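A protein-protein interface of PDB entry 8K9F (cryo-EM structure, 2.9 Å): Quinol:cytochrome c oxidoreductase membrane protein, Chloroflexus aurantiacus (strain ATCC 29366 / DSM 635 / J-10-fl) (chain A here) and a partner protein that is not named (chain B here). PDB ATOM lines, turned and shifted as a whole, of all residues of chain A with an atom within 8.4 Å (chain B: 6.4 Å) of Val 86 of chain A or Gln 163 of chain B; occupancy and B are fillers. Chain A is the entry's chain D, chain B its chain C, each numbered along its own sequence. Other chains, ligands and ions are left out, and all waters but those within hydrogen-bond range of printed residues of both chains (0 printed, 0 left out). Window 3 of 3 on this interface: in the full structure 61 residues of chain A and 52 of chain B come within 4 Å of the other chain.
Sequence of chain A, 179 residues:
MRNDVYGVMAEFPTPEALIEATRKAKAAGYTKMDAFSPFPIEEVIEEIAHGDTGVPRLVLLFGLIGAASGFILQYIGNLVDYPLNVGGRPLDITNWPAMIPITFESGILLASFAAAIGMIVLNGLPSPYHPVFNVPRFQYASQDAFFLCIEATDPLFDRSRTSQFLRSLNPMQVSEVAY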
ATOM      1  N   GLN A  74      10.755   0.266  19.760  1.00  0.00           N
ATOM      2  CA  GLN A  74      10.762  -0.229  18.384  1.00  0.00           C
ATOM      3  C   GLN A  74      12.046  -0.986  18.063  1.00  0.00           C
ATOM      4  O   GLN A  74      11.997  -2.052  17.434  1.00  0.00           O
ATOM      5  CB  GLN A  74      10.586   0.919  17.396  1.00  0.00           C
ATOM      6  CG  GLN A  74       9.256   1.601  17.455  1.00  0.00           C
ATOM      7  CD  GLN A  74       9.124   2.656  16.393  1.00  0.00           C
ATOM      8  OE1 GLN A  74       8.721   2.368  15.269  1.00  0.00           O
ATOM      9  NE2 GLN A  74       9.473   3.889  16.734  1.00  0.00           N
ATOM     10  N   GLY A  77      12.125  -4.329  20.086  1.00  0.00           N
ATOM     11  CA  GLY A  77      11.115  -5.227  19.584  1.00  0.00           C
ATOM     12  C   GLY A  77      11.413  -5.831  18.234  1.00  0.00           C
ATOM     13  O   GLY A  77      11.491  -7.056  18.113  1.00  0.00           O
ATOM     14  N   ASN A  78      11.601  -5.002  17.213  1.00  0.00           N
ATOM     15  CA  ASN A  78      11.696  -5.535  15.864  1.00  0.00           C
ATOM     16  C   ASN A  78      13.111  -5.794  15.383  1.00  0.00           C
ATOM     17  O   ASN A  78      13.270  -6.438  14.343  1.00  0.00           O
ATOM     18  CB  ASN A  78      10.999  -4.599  14.880  1.00  0.00           C
ATOM     19  CG  ASN A  78       9.519  -4.791  14.876  1.00  0.00           C
ATOM     20  OD1 ASN A  78       8.787  -3.996  15.436  1.00  0.00           O
ATOM     21  ND2 ASN A  78       9.060  -5.847  14.223  1.00  0.00           N
ATOM     22  N   LEU A  79      14.144  -5.325  16.083  1.00  0.00           N
ATOM     23  CA  LEU A  79      15.492  -5.532  15.586  1.00  0.00           C
ATOM     24  C   LEU A  79      16.392  -6.317  16.527  1.00  0.00           C
ATOM     25  O   LEU A  79      17.460  -6.759  16.094  1.00  0.00           O
ATOM     26  CB  LEU A  79      16.156  -4.185  15.250  1.00  0.00           C
ATOM     27  CG  LEU A  79      15.359  -3.197  14.389  1.00  0.00           C
ATOM     28  CD1 LEU A  79      16.156  -1.940  14.099  1.00  0.00           C
ATOM     29  CD2 LEU A  79      14.910  -3.815  13.086  1.00  0.00           C
ATOM     30  N   TYR A  82      13.227 -10.137  18.630  1.00  0.00           N
ATOM     31  CA  TYR A  82      12.753 -11.020  17.567  1.00  0.00           C
ATOM     32  C   TYR A  82      13.115 -10.383  16.237  1.00  0.00           C
ATOM     33  O   TYR A  82      12.300  -9.670  15.635  1.00  0.00           O
ATOM     34  CB  TYR A  82      11.249 -11.276  17.662  1.00  0.00           C
ATOM     35  CG  TYR A  82      10.854 -12.672  17.231  1.00  0.00           C
ATOM     36  CD1 TYR A  82      11.709 -13.448  16.457  1.00  0.00           C
ATOM     37  CD2 TYR A  82       9.639 -13.220  17.609  1.00  0.00           C
ATOM     38  CE1 TYR A  82      11.367 -14.711  16.066  1.00  0.00           C
ATOM     39  CE2 TYR A  82       9.289 -14.493  17.223  1.00  0.00           C
ATOM     40  CZ  TYR A  82      10.161 -15.232  16.449  1.00  0.00           C
ATOM     41  OH  TYR A  82       9.832 -16.505  16.053  1.00  0.00           O
ATOM     42  N   PRO A  83      14.329 -10.612  15.749  1.00  0.00           N
ATOM     43  CA  PRO A  83      14.707 -10.051  14.450  1.00  0.00           C
ATOM     44  C   PRO A  83      14.002 -10.787  13.326  1.00  0.00           C
ATOM     45  O   PRO A  83      14.349 -11.924  13.000  1.00  0.00           O
ATOM     46  CB  PRO A  83      16.229 -10.251  14.401  1.00  0.00           C
ATOM     47  CG  PRO A  83      16.626 -10.790  15.757  1.00  0.00           C
ATOM     48  CD  PRO A  83      15.408 -11.429  16.323  1.00  0.00           C
ATOM     49  N   LEU A  84      12.999 -10.146  12.739  1.00  0.00           N
ATOM     50  CA  LEU A  84      12.204 -10.736  11.676  1.00  0.00           C
ATOM     51  C   LEU A  84      12.504 -10.019  10.374  1.00  0.00           C
ATOM     52  O   LEU A  84      12.740  -8.807  10.359  1.00  0.00           O
ATOM     53  CB  LEU A  84      10.711 -10.654  11.984  1.00  0.00           C
ATOM     54  CG  LEU A  84      10.238 -11.522  13.144  1.00  0.00           C
ATOM     55  CD1 LEU A  84       8.828 -11.149  13.562  1.00  0.00           C
ATOM     56  CD2 LEU A  84      10.324 -12.990  12.769  1.00  0.00           C
ATOM     57  N   ASN A  85      12.507 -10.773   9.286  1.00  0.00           N
ATOM     58  CA  ASN A  85      12.692 -10.208   7.960  1.00  0.00           C
ATOM     59  C   ASN A  85      11.320  -9.871   7.394  1.00  0.00           C
ATOM     60  O   ASN A  85      10.549 -10.768   7.048  1.00  0.00           O
ATOM     61  CB  ASN A  85      13.440 -11.182   7.057  1.00  0.00           C
ATOM     62  CG  ASN A  85      13.893 -10.538   5.766  1.00  0.00           C
ATOM     63  OD1 ASN A  85      13.971  -9.315   5.669  1.00  0.00           O
ATOM     64  ND2 ASN A  85      14.199 -11.358   4.768  1.00  0.00           N
ATOM     65  N   VAL A  86      11.005  -8.582   7.322  1.00  0.00           N
ATOM     66  CA  VAL A  86       9.801  -8.109   6.655  1.00  0.00           C
ATOM     67  C   VAL A  86      10.235  -7.229   5.491  1.00  0.00           C
ATOM     68  O   VAL A  86      11.182  -6.446   5.616  1.00  0.00           O
ATOM     69  CB  VAL A  86       8.839  -7.376   7.614  1.00  0.00           C
ATOM     70  CG1 VAL A  86       8.340  -8.331   8.674  1.00  0.00           C
ATOM     71  CG2 VAL A  86       9.488  -6.188   8.300  1.00  0.00           C
ATOM     72  N   GLY A  87       9.626  -7.452   4.330  1.00  0.00           N
ATOM     73  CA  GLY A  87       9.744  -6.575   3.179  1.00  0.00           C
ATOM     74  C   GLY A  87      11.110  -6.337   2.573  1.00  0.00           C
ATOM     75  O   GLY A  87      11.253  -5.495   1.684  1.00  0.00           O
ATOM     76  N   GLY A  88      12.126  -7.042   3.052  1.00  0.00           N
ATOM     77  CA  GLY A  88      13.471  -6.635   2.747  1.00  0.00           C
ATOM     78  C   GLY A  88      13.931  -5.397   3.477  1.00  0.00           C
ATOM     79  O   GLY A  88      14.956  -4.825   3.103  1.00  0.00           O
ATOM     80  N   ARG A  89      13.191  -4.956   4.492  1.00  0.00           N
ATOM     81  CA  ARG A  89      13.578  -3.797   5.274  1.00  0.00           C
ATOM     82  C   ARG A  89      14.795  -4.142   6.126  1.00  0.00           C
ATOM     83  O   ARG A  89      14.982  -5.302   6.498  1.00  0.00           O
ATOM     84  CB  ARG A  89      12.421  -3.346   6.164  1.00  0.00           C
ATOM     85  CG  ARG A  89      11.093  -3.208   5.458  1.00  0.00           C
ATOM     86  CD  ARG A  89      11.165  -2.299   4.260  1.00  0.00           C
ATOM     87  NE  ARG A  89      10.691  -2.941   3.041  1.00  0.00           N
ATOM     88  CZ  ARG A  89       9.942  -2.343   2.125  1.00  0.00           C
ATOM     89  NH1 ARG A  89       9.551  -1.087   2.263  1.00  0.00           N
ATOM     90  NH2 ARG A  89       9.566  -3.025   1.047  1.00  0.00           N
ATOM     91  N   PRO A  90      15.659  -3.168   6.414  1.00  0.00           N
ATOM     92  CA  PRO A  90      16.887  -3.481   7.149  1.00  0.00           C
ATOM     93  C   PRO A  90      16.616  -3.785   8.614  1.00  0.00           C
ATOM     94  O   PRO A  90      15.596  -3.399   9.186  1.00  0.00           O
ATOM     95  CB  PRO A  90      17.734  -2.216   6.987  1.00  0.00           C
ATOM     96  CG  PRO A  90      16.766  -1.143   6.702  1.00  0.00           C
ATOM     97  CD  PRO A  90      15.644  -1.766   5.956  1.00  0.00           C
ATOM     98  N   LEU A  91      17.551  -4.519   9.214  1.00  0.00           N
ATOM     99  CA  LEU A  91      17.471  -4.893  10.619  1.00  0.00           C
ATOM    100  C   LEU A  91      18.498  -4.155  11.469  1.00  0.00           C
ATOM    101  O   LEU A  91      18.911  -4.657  12.518  1.00  0.00           O
ATOM    102  CB  LEU A  91      17.621  -6.406  10.770  1.00  0.00           C
ATOM    103  CG  LEU A  91      16.351  -7.196  10.446  1.00  0.00           C
ATOM    104  CD1 LEU A  91      16.646  -8.423   9.596  1.00  0.00           C
ATOM    105  CD2 LEU A  91      15.655  -7.600  11.728  1.00  0.00           C
ATOM    106  N   ASN A  95      17.073   1.327   9.318  1.00  0.00           N
ATOM    107  CA  ASN A  95      15.627   1.225   9.390  1.00  0.00           C
ATOM    108  C   ASN A  95      15.064   2.407  10.219  1.00  0.00           C
ATOM    109  O   ASN A  95      13.965   2.324  10.774  1.00  0.00           O
ATOM    110  CB  ASN A  95      15.313  -0.191   9.947  1.00  0.00           C
ATOM    111  CG  ASN A  95      13.840  -0.660   9.852  1.00  0.00           C
ATOM    112  OD1 ASN A  95      13.140  -0.266   8.925  1.00  0.00           O
ATOM    113  ND2 ASN A  95      13.346  -1.366  10.861  1.00  0.00           N
ATOM    114  N   ALA A  98      10.330   4.664   9.112  1.00  0.00           N
ATOM    115  CA  ALA A  98       9.374   3.724   9.703  1.00  0.00           C
ATOM    116  C   ALA A  98       9.768   3.373  11.131  1.00  0.00           C
ATOM    117  O   ALA A  98       9.478   2.276  11.614  1.00  0.00           O
ATOM    118  CB  ALA A  98       9.176   2.450   8.861  1.00  0.00           C
ATOM    119  N   MET A  99      10.433   4.298  11.809  1.00  0.00           N
ATOM    120  CA  MET A  99      10.573   4.257  13.254  1.00  0.00           C
ATOM    121  C   MET A  99      10.344   5.609  13.909  1.00  0.00           C
ATOM    122  O   MET A  99      10.144   5.665  15.123  1.00  0.00           O
ATOM    123  CB  MET A  99      11.950   3.704  13.637  1.00  0.00           C
ATOM    124  CG  MET A  99      11.863   2.280  14.159  1.00  0.00           C
ATOM    125  SD  MET A  99      13.421   1.386  14.213  1.00  0.00           S
ATOM    126  CE  MET A  99      14.499   2.664  14.795  1.00  0.00           C
ATOM    127  N   ILE A 102       6.193   6.385  15.560  1.00  0.00           N
ATOM    128  CA  ILE A 102       5.896   5.839  16.882  1.00  0.00           C
ATOM    129  C   ILE A 102       6.721   6.548  17.947  1.00  0.00           C
ATOM    130  O   ILE A 102       6.242   6.785  19.065  1.00  0.00           O
ATOM    131  CB  ILE A 102       6.108   4.316  16.875  1.00  0.00           C
ATOM    132  CG1 ILE A 102       5.206   3.703  15.807  1.00  0.00           C
ATOM    133  CG2 ILE A 102       5.856   3.698  18.238  1.00  0.00           C
ATOM    134  CD1 ILE A 102       5.116   2.226  15.832  1.00  0.00           C
ATOM    135  N   TRP B 161       5.774  -9.294  18.755  1.00  0.00           N
ATOM    136  CA  TRP B 161       5.717  -7.845  18.746  1.00  0.00           C
ATOM    137  C   TRP B 161       4.881  -7.414  17.558  1.00  0.00           C
ATOM    138  O   TRP B 161       4.727  -8.171  16.595  1.00  0.00           O
ATOM    139  CB  TRP B 161       7.120  -7.246  18.621  1.00  0.00           C
ATOM    140  CG  TRP B 161       8.033  -7.610  19.718  1.00  0.00           C
ATOM    141  CD1 TRP B 161       8.761  -8.755  19.835  1.00  0.00           C
ATOM    142  CD2 TRP B 161       8.341  -6.821  20.862  1.00  0.00           C
ATOM    143  NE1 TRP B 161       9.503  -8.728  20.985  1.00  0.00           N
ATOM    144  CE2 TRP B 161       9.265  -7.547  21.633  1.00  0.00           C
ATOM    145  CE3 TRP B 161       7.936  -5.563  21.303  1.00  0.00           C
ATOM    146  CZ2 TRP B 161       9.782  -7.061  22.822  1.00  0.00           C
ATOM    147  CZ3 TRP B 161       8.450  -5.085  22.484  1.00  0.00           C
ATOM    148  CH2 TRP B 161       9.361  -5.831  23.233  1.00  0.00           C
ATOM    149  N   PRO B 162       4.322  -6.210  17.595  1.00  0.00           N
ATOM    150  CA  PRO B 162       3.823  -5.608  16.361  1.00  0.00           C
ATOM    151  C   PRO B 162       4.985  -5.288  15.434  1.00  0.00           C
ATOM    152  O   PRO B 162       6.133  -5.151  15.858  1.00  0.00           O
ATOM    153  CB  PRO B 162       3.120  -4.338  16.838  1.00  0.00           C
ATOM    154  CG  PRO B 162       2.831  -4.581  18.266  1.00  0.00           C
ATOM    155  CD  PRO B 162       3.948  -5.421  18.777  1.00  0.00           C
ATOM    156  N   GLN B 163       4.739  -5.212  14.120  1.00  0.00           N
ATOM    157  CA  GLN B 163       5.829  -4.999  13.137  1.00  0.00           C
ATOM    158  C   GLN B 163       6.419  -3.628  13.227  1.00  0.00           C
ATOM    159  O   GLN B 163       7.584  -3.449  12.913  1.00  0.00           O
ATOM    160  CB  GLN B 163       5.378  -5.279  11.727  1.00  0.00           C
ATOM    161  CG  GLN B 163       6.468  -5.222  10.691  1.00  0.00           C
ATOM    162  CD  GLN B 163       5.961  -5.674   9.361  1.00  0.00           C
ATOM    163  OE1 GLN B 163       4.828  -6.112   9.243  1.00  0.00           O
ATOM    164  NE2 GLN B 163       6.788  -5.569   8.349  1.00  0.00           N
ATOM    165  N   PHE B 164       5.651  -2.649  13.595  1.00  0.00           N
ATOM    166  CA  PHE B 164       6.105  -1.282  13.880  1.00  0.00           C
ATOM    167  C   PHE B 164       6.663  -0.515  12.685  1.00  0.00           C
ATOM    168  O   PHE B 164       7.023   0.656  12.828  1.00  0.00           O
ATOM    169  CB  PHE B 164       7.165  -1.250  14.985  1.00  0.00           C
ATOM    170  CG  PHE B 164       6.626  -1.467  16.364  1.00  0.00           C
ATOM    171  CD1 PHE B 164       5.302  -1.210  16.662  1.00  0.00           C
ATOM    172  CD2 PHE B 164       7.458  -1.908  17.375  1.00  0.00           C
ATOM    173  CE1 PHE B 164       4.822  -1.403  17.935  1.00  0.00           C
ATOM    174  CE2 PHE B 164       6.978  -2.108  18.645  1.00  0.00           C
ATOM    175  CZ  PHE B 164       5.659  -1.857  18.923  1.00  0.00           C
ATOM    176  N   ARG B 165       6.750  -1.141  11.516  1.00  0.00           N
ATOM    177  CA  ARG B 165       7.045  -0.445  10.276  1.00  0.00           C
ATOM    178  C   ARG B 165       5.841  -0.401   9.365  1.00  0.00           C
ATOM    179  O   ARG B 165       5.860   0.319   8.364  1.00  0.00           O
ATOM    180  CB  ARG B 165       8.217  -1.105   9.545  1.00  0.00           C
ATOM    181  CG  ARG B 165       9.162  -1.833  10.462  1.00  0.00           C
ATOM    182  CD  ARG B 165      10.206  -2.607   9.700  1.00  0.00           C
ATOM    183  NE  ARG B 165      10.663  -3.761  10.463  1.00  0.00           N
ATOM    184  CZ  ARG B 165      11.865  -4.305  10.342  1.00  0.00           C
ATOM    185  NH1 ARG B 165      12.761  -3.815   9.504  1.00  0.00           N
ATOM    186  NH2 ARG B 165      12.180  -5.356  11.092  1.00  0.00           N
ATOM    187  N   SER B 166       4.811  -1.169   9.684  1.00  0.00           N
ATOM    188  CA  SER B 166       3.518  -1.008   9.057  1.00  0.00           C
ATOM    189  C   SER B 166       2.899   0.317   9.452  1.00  0.00           C
ATOM    190  O   SER B 166       3.151   0.857  10.530  1.00  0.00           O
ATOM    191  CB  SER B 166       2.593  -2.129   9.474  1.00  0.00           C
ATOM    192  OG  SER B 166       1.285  -1.916   8.984  1.00  0.00           O
ATOM    193  N   ALA B 169       0.349  -0.284  12.213  1.00  0.00           N
ATOM    194  CA  ALA B 169       1.077  -0.240  13.471  1.00  0.00           C
ATOM    195  C   ALA B 169       1.347   1.192  13.905  1.00  0.00           C
ATOM    196  O   ALA B 169       1.394   1.472  15.108  1.00  0.00           O
ATOM    197  CB  ALA B 169       2.386  -1.013  13.345  1.00  0.00           C
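The backbone carbonyl oxygen of Pro 90 of chain A is in hydrogen-bond range of the guanidinium group of Arg 165 of chain B.
The backbone carbonyl oxygen (O) of Phe 164 of chain B sits close to the backbone carbonyl oxygen (O) of Ala 98 of chain A (3.2 Å).
The side-chain amide nitrogen (ND2) of Asn 95 of chain A sits close to the guanidinium group (NH1) of Arg 165 of chain B.
O of Phe 164 of chain B sits close to OE1 of Gln 74 of chain A (3.4 Å).
O of Gln 163 of chain B sits close to OD1 of Asn 78 of chain A, 2.8 Å away.
The backbone carbonyl oxygen of Pro 162 of chain B sits close to the side-chain amide oxygen of Asn 78 of chain A.
Printed residues of chain B that touch a printed residue of chain A: Trp 161, Pro 162, Gln 163, Phe 164, Arg 165 and Ala 169.
Of the 18 printed residues of chain A, 11 touch a printed residue of chain B.
Printed residues of chain A that touch a printed residue of chain B: Gln 74, Gly 77, Asn 78, Leu 79, Leu 84, Val 86, Arg 89, Pro 90, Asn 95, Ala 98 and Ile 102.
Gly 77 of chain A touches Trp 161 of chain B.
Asn 78 of chain A touches Phe 164 of chain B.
Arg 165 of chain B touches Asn 78 of chain A.
Leu 79 of chain A touches Arg 165 of chain B (CD2 to NH2, 3.7 Å).
Leu 84 of chain A touches Arg 165 of chain B.
Gln 163 of chain B touches Val 86 of chain A.
Val 86 of chain A touches Arg 165 of chain B.
NH1 of Arg 165 of chain B touches CB of Arg 89 of chain A, 3.4 Å away.
Arg 165 of chain B touches Ala 98 of chain A (CB to CB, 3.7 Å).
Phe 164 of chain B touches Ile 102 of chain A.
Printed residues of chain B within 4 Å of Asn 78 of chain A: Pro 162 (2.9 Å), Gln 163 (2.8 Å), Phe 164 (3.1 Å) and Arg 165 (3.6 Å).
Val 86 of chain A touches just these residues of chain B: Gln 163 (2.8 Å) and Arg 165 (3.5 Å).
Gly 87 of chain A touches none of the printed residues of chain B.
Of the printed residues of chain B, Ala 98 of chain A touches Phe 164 (3.2 Å) and Arg 165 (3.7 Å).
Printed residues of chain A within 4 Å of Trp 161 of chain B: Gly 77 (3.4 Å).
Printed residues of chain A within 4 Å of Gln 163 of chain B: Asn 78 (2.8 Å) and Val 86 (2.8 Å).
Of the printed residues of chain A, Arg 165 of chain B touches Asn 78, Leu 79, Leu 84, Val 86, Arg 89, Pro 90, Asn 95 and Ala 98.
Ser 166 of chain B touches none of the printed residues of chain A.
Of the printed residues of chain A, Ala 169 of chain B touches Ile 102 (3.9 Å).
The nearest printed residue of chain B that does not touch Ala 98 of chain A is Ser 166 of chain B (5.7 Å).
The guanidinium group (NE) of Arg 89 of chain A sits at hydrogen-bond distance from the backbone carbonyl oxygen (O) of Gly 87 of chain A (2.9 Å).
O of Met 99 of chain A is in hydrogen-bond range of NE2 of Gln 74 of chain A, at 2.5 Å.
The backbone carbonyl oxygen (O) of Pro 90 of chain A lies close to the side-chain amide nitrogen (ND2) of Asn 95 of chain A, at 3.5 Å.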
